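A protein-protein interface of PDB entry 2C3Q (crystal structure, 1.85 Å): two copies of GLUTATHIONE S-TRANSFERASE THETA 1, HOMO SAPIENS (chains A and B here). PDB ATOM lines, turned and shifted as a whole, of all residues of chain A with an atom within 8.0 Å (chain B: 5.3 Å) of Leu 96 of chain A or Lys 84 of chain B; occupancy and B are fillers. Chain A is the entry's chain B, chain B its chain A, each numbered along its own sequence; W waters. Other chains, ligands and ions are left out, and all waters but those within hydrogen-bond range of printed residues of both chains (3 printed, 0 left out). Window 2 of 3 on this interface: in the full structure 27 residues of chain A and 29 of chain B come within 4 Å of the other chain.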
ATOM      1  N   PRO A  93      -9.716   7.544  19.499  1.00  0.00           N
ATOM      2  CA  PRO A  93      -9.609   8.988  19.224  1.00  0.00           C
ATOM      3  C   PRO A  93      -8.798   9.336  17.986  1.00  0.00           C
ATOM      4  O   PRO A  93      -7.816   8.640  17.699  1.00  0.00           O
ATOM      5  CB  PRO A  93      -8.901   9.518  20.476  1.00  0.00           C
ATOM      6  CG  PRO A  93      -9.252   8.580  21.523  1.00  0.00           C
ATOM      7  CD  PRO A  93      -9.226   7.239  20.860  1.00  0.00           C
ATOM      8  N   GLN A  94      -9.222  10.387  17.271  1.00  0.00           N
ATOM      9  CA  GLN A  94      -8.488  10.968  16.131  1.00  0.00           C
ATOM     10  C   GLN A  94      -7.073  11.404  16.501  1.00  0.00           C
ATOM     11  O   GLN A  94      -6.167  11.255  15.690  1.00  0.00           O
ATOM     12  CB  GLN A  94      -9.205  12.197  15.550  1.00  0.00           C
ATOM     13  CG  GLN A  94     -10.498  11.955  14.781  1.00  0.00           C
ATOM     14  CD  GLN A  94     -10.312  11.475  13.343  1.00  0.00           C
ATOM     15  OE1 GLN A  94      -9.256  11.674  12.722  1.00  0.00           O
ATOM     16  NE2 GLN A  94     -11.365  10.865  12.793  1.00  0.00           N
ATOM     17  N   ASP A  95      -6.913  11.956  17.711  1.00  0.00           N
ATOM     18  CA  ASP A  95      -5.644  12.462  18.250  1.00  0.00           C
ATOM     19  C   ASP A  95      -4.563  11.397  18.198  1.00  0.00           C
ATOM     20  O   ASP A  95      -4.746  10.312  18.737  1.00  0.00           O
ATOM     21  CB  ASP A  95      -5.810  12.949  19.694  1.00  0.00           C
ATOM     22  CG  ASP A  95      -4.502  13.435  20.303  1.00  0.00           C
ATOM     23  OD1 ASP A  95      -4.025  14.523  19.900  1.00  0.00           O
ATOM     24  OD2 ASP A  95      -3.935  12.745  21.195  1.00  0.00           O
ATOM     25  N   LEU A  96      -3.464  11.733  17.526  1.00  0.00           N
ATOM     26  CA  LEU A  96      -2.306  10.873  17.295  1.00  0.00           C
ATOM     27  C   LEU A  96      -1.839  10.097  18.529  1.00  0.00           C
ATOM     28  O   LEU A  96      -1.686   8.860  18.482  1.00  0.00           O
ATOM     29  CB  LEU A  96      -1.153  11.749  16.772  1.00  0.00           C
ATOM     30  CG  LEU A  96      -0.034  11.319  15.837  1.00  0.00           C
ATOM     31  CD1 LEU A  96      -0.534  11.180  14.402  1.00  0.00           C
ATOM     32  CD2 LEU A  96       1.080  12.328  15.872  1.00  0.00           C
ATOM     33  N   GLN A  97      -1.665  10.818  19.637  1.00  0.00           N
ATOM     34  CA  GLN A  97      -1.145  10.206  20.863  1.00  0.00           C
ATOM     35  C   GLN A  97      -2.192   9.421  21.625  1.00  0.00           C
ATOM     36  O   GLN A  97      -1.871   8.360  22.162  1.00  0.00           O
ATOM     37  CB  GLN A  97      -0.488  11.292  21.748  1.00  0.00           C
ATOM     38  CG  GLN A  97       0.820  11.790  21.072  1.00  0.00           C
ATOM     39  CD  GLN A  97       1.544  12.914  21.771  1.00  0.00           C
ATOM     40  OE1 GLN A  97       2.559  13.409  21.254  1.00  0.00           O
ATOM     41  NE2 GLN A  97       1.043  13.340  22.926  1.00  0.00           N
ATOM     42  N   ALA A  98      -3.444   9.902  21.648  1.00  0.00           N
ATOM     43  CA  ALA A  98      -4.542   9.144  22.316  1.00  0.00           C
ATOM     44  C   ALA A  98      -4.801   7.825  21.574  1.00  0.00           C
ATOM     45  O   ALA A  98      -4.888   6.774  22.203  1.00  0.00           O
ATOM     46  CB  ALA A  98      -5.817   9.970  22.456  1.00  0.00           C
ATOM     47  N   ARG A  99      -4.831   7.891  20.248  1.00  0.00           N
ATOM     48  CA  ARG A  99      -4.955   6.701  19.394  1.00  0.00           C
ATOM     49  C   ARG A  99      -3.820   5.725  19.709  1.00  0.00           C
ATOM     50  O   ARG A  99      -4.058   4.534  19.881  1.00  0.00           O
ATOM     51  CB  ARG A  99      -4.959   7.108  17.928  1.00  0.00           C
ATOM     52  CG  ARG A  99      -5.397   6.038  17.001  1.00  0.00           C
ATOM     53  CD  ARG A  99      -5.761   6.565  15.620  1.00  0.00           C
ATOM     54  NE  ARG A  99      -7.136   7.044  15.564  1.00  0.00           N
ATOM     55  CZ  ARG A  99      -7.918   7.031  14.481  1.00  0.00           C
ATOM     56  NH1 ARG A  99      -7.480   6.538  13.311  1.00  0.00           N
ATOM     57  NH2 ARG A  99      -9.169   7.481  14.574  1.00  0.00           N
ATOM     58  N   ALA A 100      -2.604   6.252  19.847  1.00  0.00           N
ATOM     59  CA  ALA A 100      -1.405   5.428  20.168  1.00  0.00           C
ATOM     60  C   ALA A 100      -1.505   4.758  21.529  1.00  0.00           C
ATOM     61  O   ALA A 100      -1.144   3.584  21.661  1.00  0.00           O
ATOM     62  CB  ALA A 100      -0.131   6.254  20.082  1.00  0.00           C
ATOM     63  N   ARG A 101      -2.023   5.477  22.534  1.00  0.00           N
ATOM     64  CA  ARG A 101      -2.258   4.849  23.834  1.00  0.00           C
ATOM     65  C   ARG A 101      -3.247   3.668  23.752  1.00  0.00           C
ATOM     66  O   ARG A 101      -3.062   2.661  24.438  1.00  0.00           O
ATOM     67  CB  ARG A 101      -2.739   5.885  24.853  1.00  0.00           C
ATOM     68  CG  ARG A 101      -1.622   6.839  25.242  1.00  0.00           C
ATOM     69  CD  ARG A 101      -2.022   7.721  26.432  1.00  0.00           C
ATOM     70  NE  ARG A 101      -3.121   8.654  26.107  1.00  0.00           N
ATOM     71  CZ  ARG A 101      -2.979   9.912  25.675  1.00  0.00           C
ATOM     72  NH1 ARG A 101      -1.775  10.463  25.508  1.00  0.00           N
ATOM     73  NH2 ARG A 101      -4.066  10.635  25.426  1.00  0.00           N
ATOM     74  N   VAL A 102      -4.270   3.788  22.906  1.00  0.00           N
ATOM     75  CA  VAL A 102      -5.236   2.706  22.708  1.00  0.00           C
ATOM     76  C   VAL A 102      -4.487   1.549  22.039  1.00  0.00           C
ATOM     77  O   VAL A 102      -4.582   0.419  22.523  1.00  0.00           O
ATOM     78  CB  VAL A 102      -6.493   3.141  21.902  1.00  0.00           C
ATOM     79  CG1 VAL A 102      -7.462   1.964  21.687  1.00  0.00           C
ATOM     80  CG2 VAL A 102      -7.209   4.272  22.593  1.00  0.00           C
ATOM     81  N   ASP A 103      -3.667   1.853  21.017  1.00  0.00           N
ATOM     82  CA  ASP A 103      -2.897   0.803  20.315  1.00  0.00           C
ATOM     83  C   ASP A 103      -1.921   0.097  21.243  1.00  0.00           C
ATOM     84  O   ASP A 103      -1.773  -1.101  21.137  1.00  0.00           O
ATOM     85  CB  ASP A 103      -2.119   1.360  19.114  1.00  0.00           C
ATOM     86  CG  ASP A 103      -3.009   1.791  17.963  1.00  0.00           C
ATOM     87  OD1 ASP A 103      -4.062   1.155  17.700  1.00  0.00           O
ATOM     88  OD2 ASP A 103      -2.585   2.740  17.264  1.00  0.00           O
ATOM     89  N   ASP B  66       9.312  10.911  21.800  1.00  0.00           N
ATOM     90  CA  ASP B  66       9.061  12.015  20.886  1.00  0.00           C
ATOM     91  C   ASP B  66       8.615  13.179  21.732  1.00  0.00           C
ATOM     92  O   ASP B  66       7.423  13.430  21.915  1.00  0.00           O
ATOM     93  CB  ASP B  66       8.021  11.584  19.842  1.00  0.00           C
ATOM     94  CG  ASP B  66       7.840  12.577  18.692  1.00  0.00           C
ATOM     95  OD1 ASP B  66       8.669  13.502  18.503  1.00  0.00           O
ATOM     96  OD2 ASP B  66       6.850  12.393  17.929  1.00  0.00           O
ATOM     97  N   LEU B  79       2.322   1.964  13.921  1.00  0.00           N
ATOM     98  CA  LEU B  79       1.116   2.740  13.588  1.00  0.00           C
ATOM     99  C   LEU B  79       1.300   4.232  13.883  1.00  0.00           C
ATOM    100  O   LEU B  79       0.872   5.057  13.081  1.00  0.00           O
ATOM    101  CB  LEU B  79      -0.126   2.182  14.314  1.00  0.00           C
ATOM    102  CG  LEU B  79      -0.632   0.823  13.866  1.00  0.00           C
ATOM    103  CD1 LEU B  79      -1.808   0.367  14.718  1.00  0.00           C
ATOM    104  CD2 LEU B  79      -0.988   0.933  12.387  1.00  0.00           C
ATOM    105  N   TYR B  80       1.948   4.581  14.998  1.00  0.00           N
ATOM    106  CA  TYR B  80       2.188   6.001  15.294  1.00  0.00           C
ATOM    107  C   TYR B  80       3.083   6.640  14.216  1.00  0.00           C
ATOM    108  O   TYR B  80       2.776   7.724  13.704  1.00  0.00           O
ATOM    109  CB  TYR B  80       2.768   6.176  16.706  1.00  0.00           C
ATOM    110  CG  TYR B  80       3.204   7.582  17.065  1.00  0.00           C
ATOM    111  CD1 TYR B  80       4.553   7.982  16.912  1.00  0.00           C
ATOM    112  CD2 TYR B  80       2.287   8.512  17.594  1.00  0.00           C
ATOM    113  CE1 TYR B  80       4.963   9.257  17.232  1.00  0.00           C
ATOM    114  CE2 TYR B  80       2.703   9.813  17.931  1.00  0.00           C
ATOM    115  CZ  TYR B  80       4.035  10.160  17.748  1.00  0.00           C
ATOM    116  OH  TYR B  80       4.450  11.417  18.068  1.00  0.00           O
ATOM    117  N   LEU B  81       4.189   5.978  13.881  1.00  0.00           N
ATOM    118  CA  LEU B  81       5.073   6.472  12.804  1.00  0.00           C
ATOM    119  C   LEU B  81       4.350   6.541  11.449  1.00  0.00           C
ATOM    120  O   LEU B  81       4.561   7.512  10.699  1.00  0.00           O
ATOM    121  CB  LEU B  81       6.341   5.609  12.702  1.00  0.00           C
ATOM    122  CG  LEU B  81       7.304   5.570  13.903  1.00  0.00           C
ATOM    123  CD1 LEU B  81       8.447   4.586  13.662  1.00  0.00           C
ATOM    124  CD2 LEU B  81       7.873   6.962  14.274  1.00  0.00           C
ATOM    125  N   THR B  82       3.472   5.563  11.177  1.00  0.00           N
ATOM    126  CA  THR B  82       2.666   5.513   9.935  1.00  0.00           C
ATOM    127  C   THR B  82       1.870   6.799   9.752  1.00  0.00           C
ATOM    128  O   THR B  82       1.926   7.447   8.701  1.00  0.00           O
ATOM    129  CB  THR B  82       1.733   4.256   9.892  1.00  0.00           C
ATOM    130  OG1 THR B  82       2.527   3.076   9.700  1.00  0.00           O
ATOM    131  CG2 THR B  82       0.703   4.337   8.779  1.00  0.00           C
ATOM    132  N   ARG B  83       1.213   7.191  10.835  1.00  0.00           N
ATOM    133  CA  ARG B  83       0.323   8.333  10.885  1.00  0.00           C
ATOM    134  C   ARG B  83       1.032   9.698  10.925  1.00  0.00           C
ATOM    135  O   ARG B  83       0.722  10.570  10.078  1.00  0.00           O
ATOM    136  CB  ARG B  83      -0.595   8.137  12.103  1.00  0.00           C
ATOM    137  CG  ARG B  83      -1.636   7.051  11.875  1.00  0.00           C
ATOM    138  CD  ARG B  83      -2.250   6.590  13.211  1.00  0.00           C
ATOM    139  NE  ARG B  83      -3.136   5.428  13.008  1.00  0.00           N
ATOM    140  CZ  ARG B  83      -3.383   4.500  13.935  1.00  0.00           C
ATOM    141  NH1 ARG B  83      -2.807   4.586  15.123  1.00  0.00           N
ATOM    142  NH2 ARG B  83      -4.200   3.478  13.670  1.00  0.00           N
ATOM    143  N   LYS B  84       1.984   9.868  11.853  1.00  0.00           N
ATOM    144  CA  LYS B  84       2.688  11.144  12.025  1.00  0.00           C
ATOM    145  C   LYS B  84       3.507  11.556  10.794  1.00  0.00           C
ATOM    146  O   LYS B  84       3.441  12.721  10.376  1.00  0.00           O
ATOM    147  CB  LYS B  84       3.600  11.103  13.265  1.00  0.00           C
ATOM    148  CG  LYS B  84       4.152  12.493  13.619  1.00  0.00           C
ATOM    149  CD  LYS B  84       5.035  12.531  14.820  1.00  0.00           C
ATOM    150  CE  LYS B  84       5.591  13.962  14.934  1.00  0.00           C
ATOM    151  NZ  LYS B  84       6.611  14.094  15.995  1.00  0.00           N
ATOM    152  N   TYR B  85       4.185  10.599  10.169  1.00  0.00           N
ATOM    153  CA  TYR B  85       5.113  10.899   9.057  1.00  0.00           C
ATOM    154  C   TYR B  85       4.525  10.724   7.633  1.00  0.00           C
ATOM    155  O   TYR B  85       5.245  10.899   6.647  1.00  0.00           O
ATOM    156  CB  TYR B  85       6.399  10.066   9.264  1.00  0.00           C
ATOM    157  CG  TYR B  85       7.136  10.566  10.501  1.00  0.00           C
ATOM    158  CD1 TYR B  85       6.998   9.918  11.739  1.00  0.00           C
ATOM    159  CD2 TYR B  85       7.940  11.724  10.435  1.00  0.00           C
ATOM    160  CE1 TYR B  85       7.635  10.412  12.885  1.00  0.00           C
ATOM    161  CE2 TYR B  85       8.586  12.230  11.587  1.00  0.00           C
ATOM    162  CZ  TYR B  85       8.431  11.562  12.796  1.00  0.00           C
ATOM    163  OH  TYR B  85       9.068  12.036  13.934  1.00  0.00           O
ATOM    164  N   LYS B  86       3.240  10.388   7.555  1.00  0.00           N
ATOM    165  CA  LYS B  86       2.448  10.295   6.307  1.00  0.00           C
ATOM    166  C   LYS B  86       3.151   9.444   5.255  1.00  0.00           C
ATOM    167  O   LYS B  86       3.350   9.860   4.104  1.00  0.00           O
ATOM    168  CB  LYS B  86       2.125  11.691   5.736  1.00  0.00           C
ATOM    169  CG  LYS B  86       1.383  12.664   6.644  1.00  0.00           C
ATOM    170  CD  LYS B  86       1.320  14.026   5.930  1.00  0.00           C
ATOM    171  CE  LYS B  86       0.719  15.148   6.758  1.00  0.00           C
ATOM    172  NZ  LYS B  86      -0.769  15.004   6.874  1.00  0.00           N
HETATM  173  O   HOH W   1       5.478  15.211  20.800  1.00  0.00           O
HETATM  174  O   HOH W   2      -1.017   6.634  16.584  1.00  0.00           O
HETATM  175  O   HOH W   3      -0.300   4.037  17.380  1.00  0.00           O
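OD2 of Asp 103 of chain A lies within salt-bridge range of NH1 of Arg 83 of chain B (2.8 Å).
Water W3 lies within hydrogen-bond range of OD2 of Asp 103 of chain A (2.6 Å), N of Tyr 80 of chain B (3.3 Å) and NH1 of Arg 83 of chain B (3.4 Å).
Water W1 lies within hydrogen-bond range of O of Asp 66 of chain B (2.9 Å) and OE1 of Gln 97 of chain A (3.5 Å).
Water W2 lies within hydrogen-bond range of the backbone carbonyl oxygen (O) of Leu 96 of chain A (3.0 Å) and the guanidinium group (NH1) of Arg 83 of chain B (3.1 Å).
Of the printed residues of chain B, Arg 99 of chain A touches Arg 83.
Ala 100 of chain A touches none of the printed residues of chain B.
Val 102 of chain A touches none of the printed residues of chain B.
Printed residues of chain B within 4 Å of Asp 103 of chain A: Leu 79 and Arg 83.
Of the printed residues of chain A, Tyr 80 of chain B touches Leu 96 (3.6 Å).
Printed residues of chain A within 4 Å of Arg 83 of chain B: Leu 96 (3.8 Å), Arg 99 (3.5 Å) and Asp 103 (2.8 Å).
Of chain A, only Leu 96 comes within 4 Å of Lys 84 of chain B.
The nearest printed residue of chain B that does not touch Leu 96 of chain A is Asp 66 of chain B (6.1 Å).
The nearest printed residue of chain B that does not touch Arg 99 of chain A is Leu 79 of chain B (7.0 Å).
Printed residues of chain B that touch a printed residue of chain A: Leu 79, Tyr 80, Arg 83 and Lys 84.
Hydrophobic or aromatic side chains of chain B within 4 Å of the printed part of chain A: Leu 79 and Tyr 80.
Along chain B the printed residues that touch a printed residue of chain A span positions 79 to 84.
Among the printed residues, Asp or Glu carboxylates within 4 Å of a Lys or Arg side-chain nitrogen of the other chain: Asp 103 of chain A with Arg 83 of chain B.
No position is printed for both chains.
Of the 6 pairs that touch across the chains among the printed residues, none has its exchanged pair printed and touching as well.
OH of Tyr 80 of chain B lies within hydrogen-bond range of OD2 of Asp 66 of chain B (2.6 Å).
The side-chain amino group of Lys 84 of chain B is in salt-bridge range of the side-chain carboxylate of Asp 66 of chain B (2.6 Å).
The backbone carbonyl oxygen (O) of Pro 93 of chain A is in hydrogen-bond range of the guanidinium group (NE) of Arg 99 of chain A (2.8 Å).
Tyr 80 of chain B touches Leu 96 of chain A (CE2 to CD2, 3.6 Å).
Leu 96 of chain A touches Arg 83 of chain B (CD1 to CB, 3.8 Å).
CD2 of Leu 96 of chain A touches CG of Lys 84 of chain B, 3.8 Å away.
Arg 99 of chain A touches Arg 83 of chain B (CG to NH1, 3.5 Å).
OD2 of Asp 103 of chain A touches CD1 of Leu 79 of chain B, 3.6 Å away.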
